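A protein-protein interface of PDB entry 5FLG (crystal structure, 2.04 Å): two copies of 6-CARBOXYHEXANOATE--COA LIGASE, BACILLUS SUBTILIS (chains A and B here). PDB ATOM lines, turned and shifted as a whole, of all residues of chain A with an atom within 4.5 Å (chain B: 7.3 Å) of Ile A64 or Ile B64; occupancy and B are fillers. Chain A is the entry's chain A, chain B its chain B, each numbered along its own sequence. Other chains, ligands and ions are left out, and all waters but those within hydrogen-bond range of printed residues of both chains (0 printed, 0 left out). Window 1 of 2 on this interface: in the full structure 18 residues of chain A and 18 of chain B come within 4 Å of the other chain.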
ATOM      1  N   VAL A  11     -32.044  -2.021  18.235  1.00  0.00           N
ATOM      2  CA  VAL A  11     -30.650  -1.534  18.296  1.00  0.00           C
ATOM      3  C   VAL A  11     -29.752  -2.736  18.327  1.00  0.00           C
ATOM      4  O   VAL A  11     -29.886  -3.592  19.215  1.00  0.00           O
ATOM      5  CB  VAL A  11     -30.357  -0.662  19.540  1.00  0.00           C
ATOM      6  CG1 VAL A  11     -29.007   0.021  19.382  1.00  0.00           C
ATOM      7  CG2 VAL A  11     -31.414   0.406  19.737  1.00  0.00           C
ATOM      8  N   ARG A  12     -28.901  -2.853  17.306  1.00  0.00           N
ATOM      9  CA  ARG A  12     -28.073  -4.029  17.128  1.00  0.00           C
ATOM     10  C   ARG A  12     -26.608  -3.657  17.025  1.00  0.00           C
ATOM     11  O   ARG A  12     -26.264  -2.558  16.565  1.00  0.00           O
ATOM     12  CB  ARG A  12     -28.471  -4.781  15.842  1.00  0.00           C
ATOM     13  CG  ARG A  12     -29.823  -5.464  15.951  1.00  0.00           C
ATOM     14  CD  ARG A  12     -30.150  -6.227  14.668  1.00  0.00           C
ATOM     15  NE  ARG A  12     -30.366  -5.313  13.551  1.00  0.00           N
ATOM     16  CZ  ARG A  12     -30.352  -5.676  12.271  1.00  0.00           C
ATOM     17  NH1 ARG A  12     -29.926  -6.880  11.925  1.00  0.00           N
ATOM     18  NH2 ARG A  12     -30.723  -4.820  11.337  1.00  0.00           N
ATOM     19  N   MET A  13     -25.764  -4.601  17.426  1.00  0.00           N
ATOM     20  CA  MET A  13     -24.337  -4.405  17.449  1.00  0.00           C
ATOM     21  C   MET A  13     -23.679  -5.714  17.063  1.00  0.00           C
ATOM     22  O   MET A  13     -24.021  -6.757  17.582  1.00  0.00           O
ATOM     23  CB  MET A  13     -23.847  -3.989  18.855  1.00  0.00           C
ATOM     24  CG  MET A  13     -22.323  -3.841  18.982  1.00  0.00           C
ATOM     25  SD  MET A  13     -21.422  -5.350  19.461  1.00  0.00           S
ATOM     26  CE  MET A  13     -22.036  -5.644  21.100  1.00  0.00           C
ATOM     27  N   VAL A  44     -27.060   2.447  23.250  1.00  0.00           N
ATOM     28  CA  VAL A  44     -25.922   2.474  22.369  1.00  0.00           C
ATOM     29  C   VAL A  44     -24.627   2.382  23.176  1.00  0.00           C
ATOM     30  O   VAL A  44     -23.713   1.639  22.802  1.00  0.00           O
ATOM     31  CB  VAL A  44     -25.943   3.732  21.492  1.00  0.00           C
ATOM     32  CG1 VAL A  44     -24.638   3.887  20.743  1.00  0.00           C
ATOM     33  CG2 VAL A  44     -27.107   3.662  20.508  1.00  0.00           C
ATOM     34  N   LEU A  48     -21.882  -0.567  23.008  1.00  0.00           N
ATOM     35  CA  LEU A  48     -20.482  -0.221  22.751  1.00  0.00           C
ATOM     36  C   LEU A  48     -19.609  -0.900  23.786  1.00  0.00           C
ATOM     37  O   LEU A  48     -18.669  -1.617  23.441  1.00  0.00           O
ATOM     38  CB  LEU A  48     -20.278   1.289  22.776  1.00  0.00           C
ATOM     39  CG  LEU A  48     -18.850   1.789  22.550  1.00  0.00           C
ATOM     40  CD1 LEU A  48     -18.319   1.333  21.208  1.00  0.00           C
ATOM     41  CD2 LEU A  48     -18.817   3.306  22.648  1.00  0.00           C
ATOM     42  N   MET A  62     -16.513  -2.715  14.507  1.00  0.00           N
ATOM     43  CA  MET A  62     -17.806  -2.779  15.176  1.00  0.00           C
ATOM     44  C   MET A  62     -18.818  -1.955  14.419  1.00  0.00           C
ATOM     45  O   MET A  62     -18.494  -0.917  13.858  1.00  0.00           O
ATOM     46  CB  MET A  62     -17.699  -2.311  16.633  1.00  0.00           C
ATOM     47  CG  MET A  62     -19.003  -2.386  17.410  1.00  0.00           C
ATOM     48  SD  MET A  62     -18.930  -1.659  19.077  1.00  0.00           S
ATOM     49  CE  MET A  62     -17.477  -2.498  19.718  1.00  0.00           C
ATOM     50  N   GLN A  63     -20.036  -2.490  14.345  1.00  0.00           N
ATOM     51  CA  GLN A  63     -21.193  -1.792  13.839  1.00  0.00           C
ATOM     52  C   GLN A  63     -22.281  -1.710  14.895  1.00  0.00           C
ATOM     53  O   GLN A  63     -22.612  -2.700  15.534  1.00  0.00           O
ATOM     54  CB  GLN A  63     -21.773  -2.548  12.651  1.00  0.00           C
ATOM     55  CG  GLN A  63     -20.808  -2.703  11.506  1.00  0.00           C
ATOM     56  CD  GLN A  63     -21.467  -3.322  10.258  1.00  0.00           C
ATOM     57  OE1 GLN A  63     -21.962  -4.458  10.287  1.00  0.00           O
ATOM     58  NE2 GLN A  63     -21.405  -2.601   9.148  1.00  0.00           N
ATOM     59  N   ILE A  64     -22.977  -0.586  14.943  1.00  0.00           N
ATOM     60  CA  ILE A  64     -24.116  -0.424  15.829  1.00  0.00           C
ATOM     61  C   ILE A  64     -25.139   0.283  14.994  1.00  0.00           C
ATOM     62  O   ILE A  64     -24.820   1.228  14.288  1.00  0.00           O
ATOM     63  CB  ILE A  64     -23.804   0.489  17.058  1.00  0.00           C
ATOM     64  CG1 ILE A  64     -22.615  -0.027  17.838  1.00  0.00           C
ATOM     65  CG2 ILE A  64     -25.011   0.562  17.951  1.00  0.00           C
ATOM     66  CD1 ILE A  64     -22.341   0.709  19.154  1.00  0.00           C
ATOM     67  N   GLN A  65     -26.365  -0.222  15.013  1.00  0.00           N
ATOM     68  CA  GLN A  65     -27.412   0.300  14.169  1.00  0.00           C
ATOM     69  C   GLN A  65     -28.712   0.398  14.974  1.00  0.00           C
ATOM     70  O   GLN A  65     -29.010  -0.475  15.777  1.00  0.00           O
ATOM     71  CB  GLN A  65     -27.588  -0.624  12.969  1.00  0.00           C
ATOM     72  CG  GLN A  65     -28.835  -0.348  12.149  1.00  0.00           C
ATOM     73  CD  GLN A  65     -29.109  -1.425  11.103  1.00  0.00           C
ATOM     74  OE1 GLN A  65     -30.198  -2.012  11.064  1.00  0.00           O
ATOM     75  NE2 GLN A  65     -28.133  -1.668  10.243  1.00  0.00           N
ATOM     76  N   VAL B  11     -14.162   6.247  12.250  1.00  0.00           N
ATOM     77  CA  VAL B  11     -15.472   6.132  12.884  1.00  0.00           C
ATOM     78  C   VAL B  11     -16.451   6.922  12.059  1.00  0.00           C
ATOM     79  O   VAL B  11     -16.166   8.075  11.714  1.00  0.00           O
ATOM     80  CB  VAL B  11     -15.486   6.644  14.328  1.00  0.00           C
ATOM     81  CG1 VAL B  11     -16.768   6.205  15.017  1.00  0.00           C
ATOM     82  CG2 VAL B  11     -14.299   6.102  15.103  1.00  0.00           C
ATOM     83  N   ARG B  12     -17.460   6.214  11.540  1.00  0.00           N
ATOM     84  CA  ARG B  12     -18.394   6.797  10.600  1.00  0.00           C
ATOM     85  C   ARG B  12     -19.822   6.627  11.107  1.00  0.00           C
ATOM     86  O   ARG B  12     -20.134   5.667  11.812  1.00  0.00           O
ATOM     87  CB  ARG B  12     -18.269   6.123   9.237  1.00  0.00           C
ATOM     88  CG  ARG B  12     -16.958   6.445   8.538  1.00  0.00           C
ATOM     89  CD  ARG B  12     -16.833   5.726   7.194  1.00  0.00           C
ATOM     90  NE  ARG B  12     -16.634   4.282   7.340  1.00  0.00           N
ATOM     91  CZ  ARG B  12     -17.004   3.390   6.421  1.00  0.00           C
ATOM     92  NH1 ARG B  12     -17.595   3.788   5.308  1.00  0.00           N
ATOM     93  NH2 ARG B  12     -16.800   2.106   6.616  1.00  0.00           N
ATOM     94  N   MET B  13     -20.681   7.570  10.736  1.00  0.00           N
ATOM     95  CA  MET B  13     -22.076   7.558  11.150  1.00  0.00           C
ATOM     96  C   MET B  13     -22.921   8.049  10.007  1.00  0.00           C
ATOM     97  O   MET B  13     -22.571   9.013   9.320  1.00  0.00           O
ATOM     98  CB  MET B  13     -22.315   8.477  12.353  1.00  0.00           C
ATOM     99  CG  MET B  13     -23.788   8.612  12.770  1.00  0.00           C
ATOM    100  SD  MET B  13     -24.707   9.962  11.955  1.00  0.00           S
ATOM    101  CE  MET B  13     -23.831  11.430  12.562  1.00  0.00           C
ATOM    102  N   ARG B  14     -24.108   7.486   9.891  1.00  0.00           N
ATOM    103  CA  ARG B  14     -25.095   8.120   9.077  1.00  0.00           C
ATOM    104  C   ARG B  14     -26.482   7.919   9.680  1.00  0.00           C
ATOM    105  O   ARG B  14     -26.750   6.911  10.351  1.00  0.00           O
ATOM    106  CB  ARG B  14     -25.018   7.571   7.664  1.00  0.00           C
ATOM    107  CG  ARG B  14     -25.328   6.100   7.558  1.00  0.00           C
ATOM    108  CD  ARG B  14     -25.040   5.600   6.150  1.00  0.00           C
ATOM    109  NE  ARG B  14     -25.917   4.489   5.813  1.00  0.00           N
ATOM    110  CZ  ARG B  14     -25.495   3.302   5.400  1.00  0.00           C
ATOM    111  NH1 ARG B  14     -24.203   3.104   5.146  1.00  0.00           N
ATOM    112  NH2 ARG B  14     -26.372   2.328   5.204  1.00  0.00           N
ATOM    113  N   MET B  40     -12.450   6.428  21.552  1.00  0.00           N
ATOM    114  CA  MET B  40     -13.589   5.791  20.861  1.00  0.00           C
ATOM    115  C   MET B  40     -14.934   6.124  21.515  1.00  0.00           C
ATOM    116  O   MET B  40     -15.930   6.455  20.837  1.00  0.00           O
ATOM    117  CB  MET B  40     -13.401   4.279  20.852  1.00  0.00           C
ATOM    118  CG  MET B  40     -14.410   3.534  19.976  1.00  0.00           C
ATOM    119  SD  MET B  40     -14.460   4.140  18.282  1.00  0.00           S
ATOM    120  CE  MET B  40     -13.068   3.280  17.613  1.00  0.00           C
ATOM    121  N   THR B  43     -16.007   9.646  20.946  1.00  0.00           N
ATOM    122  CA  THR B  43     -16.243   9.943  19.534  1.00  0.00           C
ATOM    123  C   THR B  43     -17.573   9.320  19.106  1.00  0.00           C
ATOM    124  O   THR B  43     -18.371   9.953  18.418  1.00  0.00           O
ATOM    125  CB  THR B  43     -15.108   9.360  18.694  1.00  0.00           C
ATOM    126  OG1 THR B  43     -13.884   9.988  19.054  1.00  0.00           O
ATOM    127  CG2 THR B  43     -15.366   9.541  17.220  1.00  0.00           C
ATOM    128  N   VAL B  44     -17.823   8.090  19.547  1.00  0.00           N
ATOM    129  CA  VAL B  44     -19.101   7.431  19.232  1.00  0.00           C
ATOM    130  C   VAL B  44     -20.270   8.193  19.831  1.00  0.00           C
ATOM    131  O   VAL B  44     -21.284   8.399  19.174  1.00  0.00           O
ATOM    132  CB  VAL B  44     -19.123   5.985  19.700  1.00  0.00           C
ATOM    133  CG1 VAL B  44     -20.528   5.423  19.595  1.00  0.00           C
ATOM    134  CG2 VAL B  44     -18.135   5.151  18.885  1.00  0.00           C
ATOM    135  N   ASN B  45     -20.038   8.780  21.005  1.00  0.00           N
ATOM    136  CA  ASN B  45     -21.028   9.629  21.615  1.00  0.00           C
ATOM    137  C   ASN B  45     -21.219  10.975  20.947  1.00  0.00           C
ATOM    138  O   ASN B  45     -22.361  11.423  20.777  1.00  0.00           O
ATOM    139  CB  ASN B  45     -20.746   9.800  23.106  1.00  0.00           C
ATOM    140  CG  ASN B  45     -21.318   8.652  23.914  1.00  0.00           C
ATOM    141  OD1 ASN B  45     -22.536   8.514  23.998  1.00  0.00           O
ATOM    142  ND2 ASN B  45     -20.470   7.726  24.322  1.00  0.00           N
ATOM    143  N   ALA B  46     -20.139  11.534  20.410  1.00  0.00           N
ATOM    144  CA  ALA B  46     -20.268  12.785  19.681  1.00  0.00           C
ATOM    145  C   ALA B  46     -21.059  12.564  18.400  1.00  0.00           C
ATOM    146  O   ALA B  46     -21.859  13.396  18.029  1.00  0.00           O
ATOM    147  CB  ALA B  46     -18.902  13.417  19.369  1.00  0.00           C
ATOM    148  N   LEU B  47     -20.748  11.503  17.680  1.00  0.00           N
ATOM    149  CA  LEU B  47     -21.495  11.178  16.458  1.00  0.00           C
ATOM    150  C   LEU B  47     -22.953  10.838  16.727  1.00  0.00           C
ATOM    151  O   LEU B  47     -23.827  11.317  16.023  1.00  0.00           O
ATOM    152  CB  LEU B  47     -20.837  10.051  15.699  1.00  0.00           C
ATOM    153  CG  LEU B  47     -19.512  10.436  15.063  1.00  0.00           C
ATOM    154  CD1 LEU B  47     -18.753   9.195  14.593  1.00  0.00           C
ATOM    155  CD2 LEU B  47     -19.730  11.380  13.893  1.00  0.00           C
ATOM    156  N   LEU B  48     -23.227  10.046  17.746  1.00  0.00           N
ATOM    157  CA  LEU B  48     -24.617   9.771  18.128  1.00  0.00           C
ATOM    158  C   LEU B  48     -25.409  11.060  18.382  1.00  0.00           C
ATOM    159  O   LEU B  48     -26.499  11.257  17.829  1.00  0.00           O
ATOM    160  CB  LEU B  48     -24.655   8.911  19.380  1.00  0.00           C
ATOM    161  CG  LEU B  48     -26.044   8.553  19.907  1.00  0.00           C
ATOM    162  CD1 LEU B  48     -26.832   7.759  18.862  1.00  0.00           C
ATOM    163  CD2 LEU B  48     -25.910   7.757  21.193  1.00  0.00           C
ATOM    164  N   GLU B  49     -24.814  11.972  19.154  1.00  0.00           N
ATOM    165  CA  GLU B  49     -25.482  13.189  19.545  1.00  0.00           C
ATOM    166  C   GLU B  49     -25.684  14.111  18.359  1.00  0.00           C
ATOM    167  O   GLU B  49     -26.724  14.763  18.241  1.00  0.00           O
ATOM    168  CB  GLU B  49     -24.697  13.911  20.657  1.00  0.00           C
ATOM    169  CG  GLU B  49     -25.157  15.344  20.933  1.00  0.00           C
ATOM    170  CD  GLU B  49     -26.625  15.471  21.377  1.00  0.00           C
ATOM    171  OE1 GLU B  49     -27.423  14.528  21.152  1.00  0.00           O
ATOM    172  OE2 GLU B  49     -27.010  16.550  21.894  1.00  0.00           O
ATOM    173  N   MET B  62     -30.131   4.833  12.191  1.00  0.00           N
ATOM    174  CA  MET B  62     -28.760   5.285  12.274  1.00  0.00           C
ATOM    175  C   MET B  62     -27.778   4.150  12.349  1.00  0.00           C
ATOM    176  O   MET B  62     -28.052   3.122  12.960  1.00  0.00           O
ATOM    177  CB  MET B  62     -28.599   6.214  13.476  1.00  0.00           C
ATOM    178  CG  MET B  62     -27.174   6.721  13.599  1.00  0.00           C
ATOM    179  SD  MET B  62     -26.946   7.594  15.146  1.00  0.00           S
ATOM    180  CE  MET B  62     -28.242   8.818  15.019  1.00  0.00           C
ATOM    181  N   GLN B  63     -26.656   4.305  11.654  1.00  0.00           N
ATOM    182  CA  GLN B  63     -25.550   3.369  11.758  1.00  0.00           C
ATOM    183  C   GLN B  63     -24.278   4.064  12.219  1.00  0.00           C
ATOM    184  O   GLN B  63     -23.882   5.058  11.641  1.00  0.00           O
ATOM    185  CB  GLN B  63     -25.208   2.774  10.422  1.00  0.00           C
ATOM    186  CG  GLN B  63     -26.270   1.922   9.792  1.00  0.00           C
ATOM    187  CD  GLN B  63     -25.644   1.090   8.686  1.00  0.00           C
ATOM    188  OE1 GLN B  63     -24.411   0.927   8.649  1.00  0.00           O
ATOM    189  NE2 GLN B  63     -26.462   0.625   7.746  1.00  0.00           N
ATOM    190  N   ILE B  64     -23.557   3.417  13.106  1.00  0.00           N
ATOM    191  CA  ILE B  64     -22.253   3.905  13.508  1.00  0.00           C
ATOM    192  C   ILE B  64     -21.321   2.734  13.410  1.00  0.00           C
ATOM    193  O   ILE B  64     -21.665   1.642  13.810  1.00  0.00           O
ATOM    194  CB  ILE B  64     -22.243   4.420  14.951  1.00  0.00           C
ATOM    195  CG1 ILE B  64     -23.337   5.464  15.161  1.00  0.00           C
ATOM    196  CG2 ILE B  64     -20.887   5.029  15.276  1.00  0.00           C
ATOM    197  CD1 ILE B  64     -23.306   6.134  16.524  1.00  0.00           C
ATOM    198  N   GLN B  65     -20.150   2.962  12.839  1.00  0.00           N
ATOM    199  CA  GLN B  65     -19.226   1.895  12.590  1.00  0.00           C
ATOM    200  C   GLN B  65     -17.811   2.401  12.899  1.00  0.00           C
ATOM    201  O   GLN B  65     -17.513   3.583  12.692  1.00  0.00           O
ATOM    202  CB  GLN B  65     -19.334   1.486  11.128  1.00  0.00           C
ATOM    203  CG  GLN B  65     -18.279   0.471  10.736  1.00  0.00           C
ATOM    204  CD  GLN B  65     -18.314   0.104   9.276  1.00  0.00           C
ATOM    205  OE1 GLN B  65     -19.357  -0.271   8.745  1.00  0.00           O
ATOM    206  NE2 GLN B  65     -17.147   0.124   8.642  1.00  0.00           N
ATOM    207  N   PHE B  66     -16.963   1.512  13.400  1.00  0.00           N
ATOM    208  CA  PHE B  66     -15.548   1.790  13.450  1.00  0.00           C
ATOM    209  C   PHE B  66     -14.735   0.635  12.916  1.00  0.00           C
ATOM    210  O   PHE B  66     -15.193  -0.500  12.888  1.00  0.00           O
ATOM    211  CB  PHE B  66     -15.075   2.255  14.841  1.00  0.00           C
ATOM    212  CG  PHE B  66     -14.931   1.148  15.859  1.00  0.00           C
ATOM    213  CD1 PHE B  66     -13.962   0.184  15.715  1.00  0.00           C
ATOM    214  CD2 PHE B  66     -15.654   1.183  17.026  1.00  0.00           C
ATOM    215  CE1 PHE B  66     -13.744  -0.750  16.693  1.00  0.00           C
ATOM    216  CE2 PHE B  66     -15.477   0.218  18.019  1.00  0.00           C
ATOM    217  CZ  PHE B  66     -14.492  -0.722  17.871  1.00  0.00           C
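The side-chain amide nitrogen of Gln A63 is in hydrogen-bond range of the side-chain amide oxygen of Gln B65, 3.1 Å away.
The backbone carbonyl oxygen of Met A62 lies within hydrogen-bond range of the backbone NH of Phe B66 (2.9 Å).
The backbone NH (N) of Ile B64 is in hydrogen-bond range of the backbone carbonyl oxygen (O) of Ile A64, 2.8 Å away.
Among the printed residues, merely in contact across the chains: Leu A48 with Val B44 (3.995 Å), Met A62 with Gln B65 (3.2 Å), Gln A63 with Ile B64 (3.5 Å), Ile A64 with Met B62 (3.97 Å), Ile A64 with Gln B63 (3.4 Å), Gln A65 with Met B62 (3.1 Å) and Gln A65 with Gln B63 (3.8 Å).
Of the 17 printed residues of chain B, 6 touch a printed residue of chain A.
Hydrophobic or aromatic side chains of chain B within 4 Å of the printed part of chain A: Val B44 and Phe B66.
Of the 9 printed residues of chain A, 5 touch a printed residue of chain B.
Among the printed residues, no Asp or Glu carboxylate lies within 4 Å of a Lys or Arg side-chain nitrogen of the other chain.
Leu A48 touches Val B44, but with the chains exchanged Val A44 does not touch Leu B48 (4.04 Å).
Gln A63 touches Gln B65, and with the chains exchanged Gln A65 touches Gln B63.
Ile A64 touches Met B62, but with the chains exchanged Met A62 does not touch Ile B64 (4.1 Å).
Ile A64 touches its own counterpart, Ile B64.
Positions printed for both chains: 11, 12, 13, 44, 48, 62, 63, 64 and 65.
Of the 10 pairs that touch across the chains among the printed residues, 7 have their exchanged pair printed and touching as well.
Printed residues of chain B within 4 Å of Leu A48: Val B44.
Of chain B, only Met B62 (3.97 Å), Gln B63 (3.4 Å) and Ile B64 (2.8 Å) come within 4 Å of Ile A64.
Of the printed residues of chain A, Met B62 touches Ile A64 (3.97 Å) and Gln A65 (3.1 Å).
Printed residues of chain A within 4 Å of Gln B63: Ile A64 (3.4 Å) and Gln A65 (3.8 Å).
Ile B64 touches just these residues of chain A: Gln A63 (3.5 Å) and Ile A64 (2.8 Å).
Of the printed residues of chain A, Phe B66 touches Met A62.
The nearest residue of chain A that does not touch Ile B64 is Met A62 (4.1 Å).
The nearest printed residue of chain A that does not touch Gln B65 is Ile A64 (5.0 Å).
The backbone NH (N) of Gln B63 is in hydrogen-bond range of the backbone carbonyl oxygen (O) of Arg B14 (2.9 Å).
The side-chain amide nitrogen (NE2) of Gln B65 sits close to the guanidinium group (NH2) of Arg B12.
The backbone carbonyl oxygen (O) of Arg A12 is in hydrogen-bond range of the backbone NH (N) of Gln A65 (2.8 Å).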
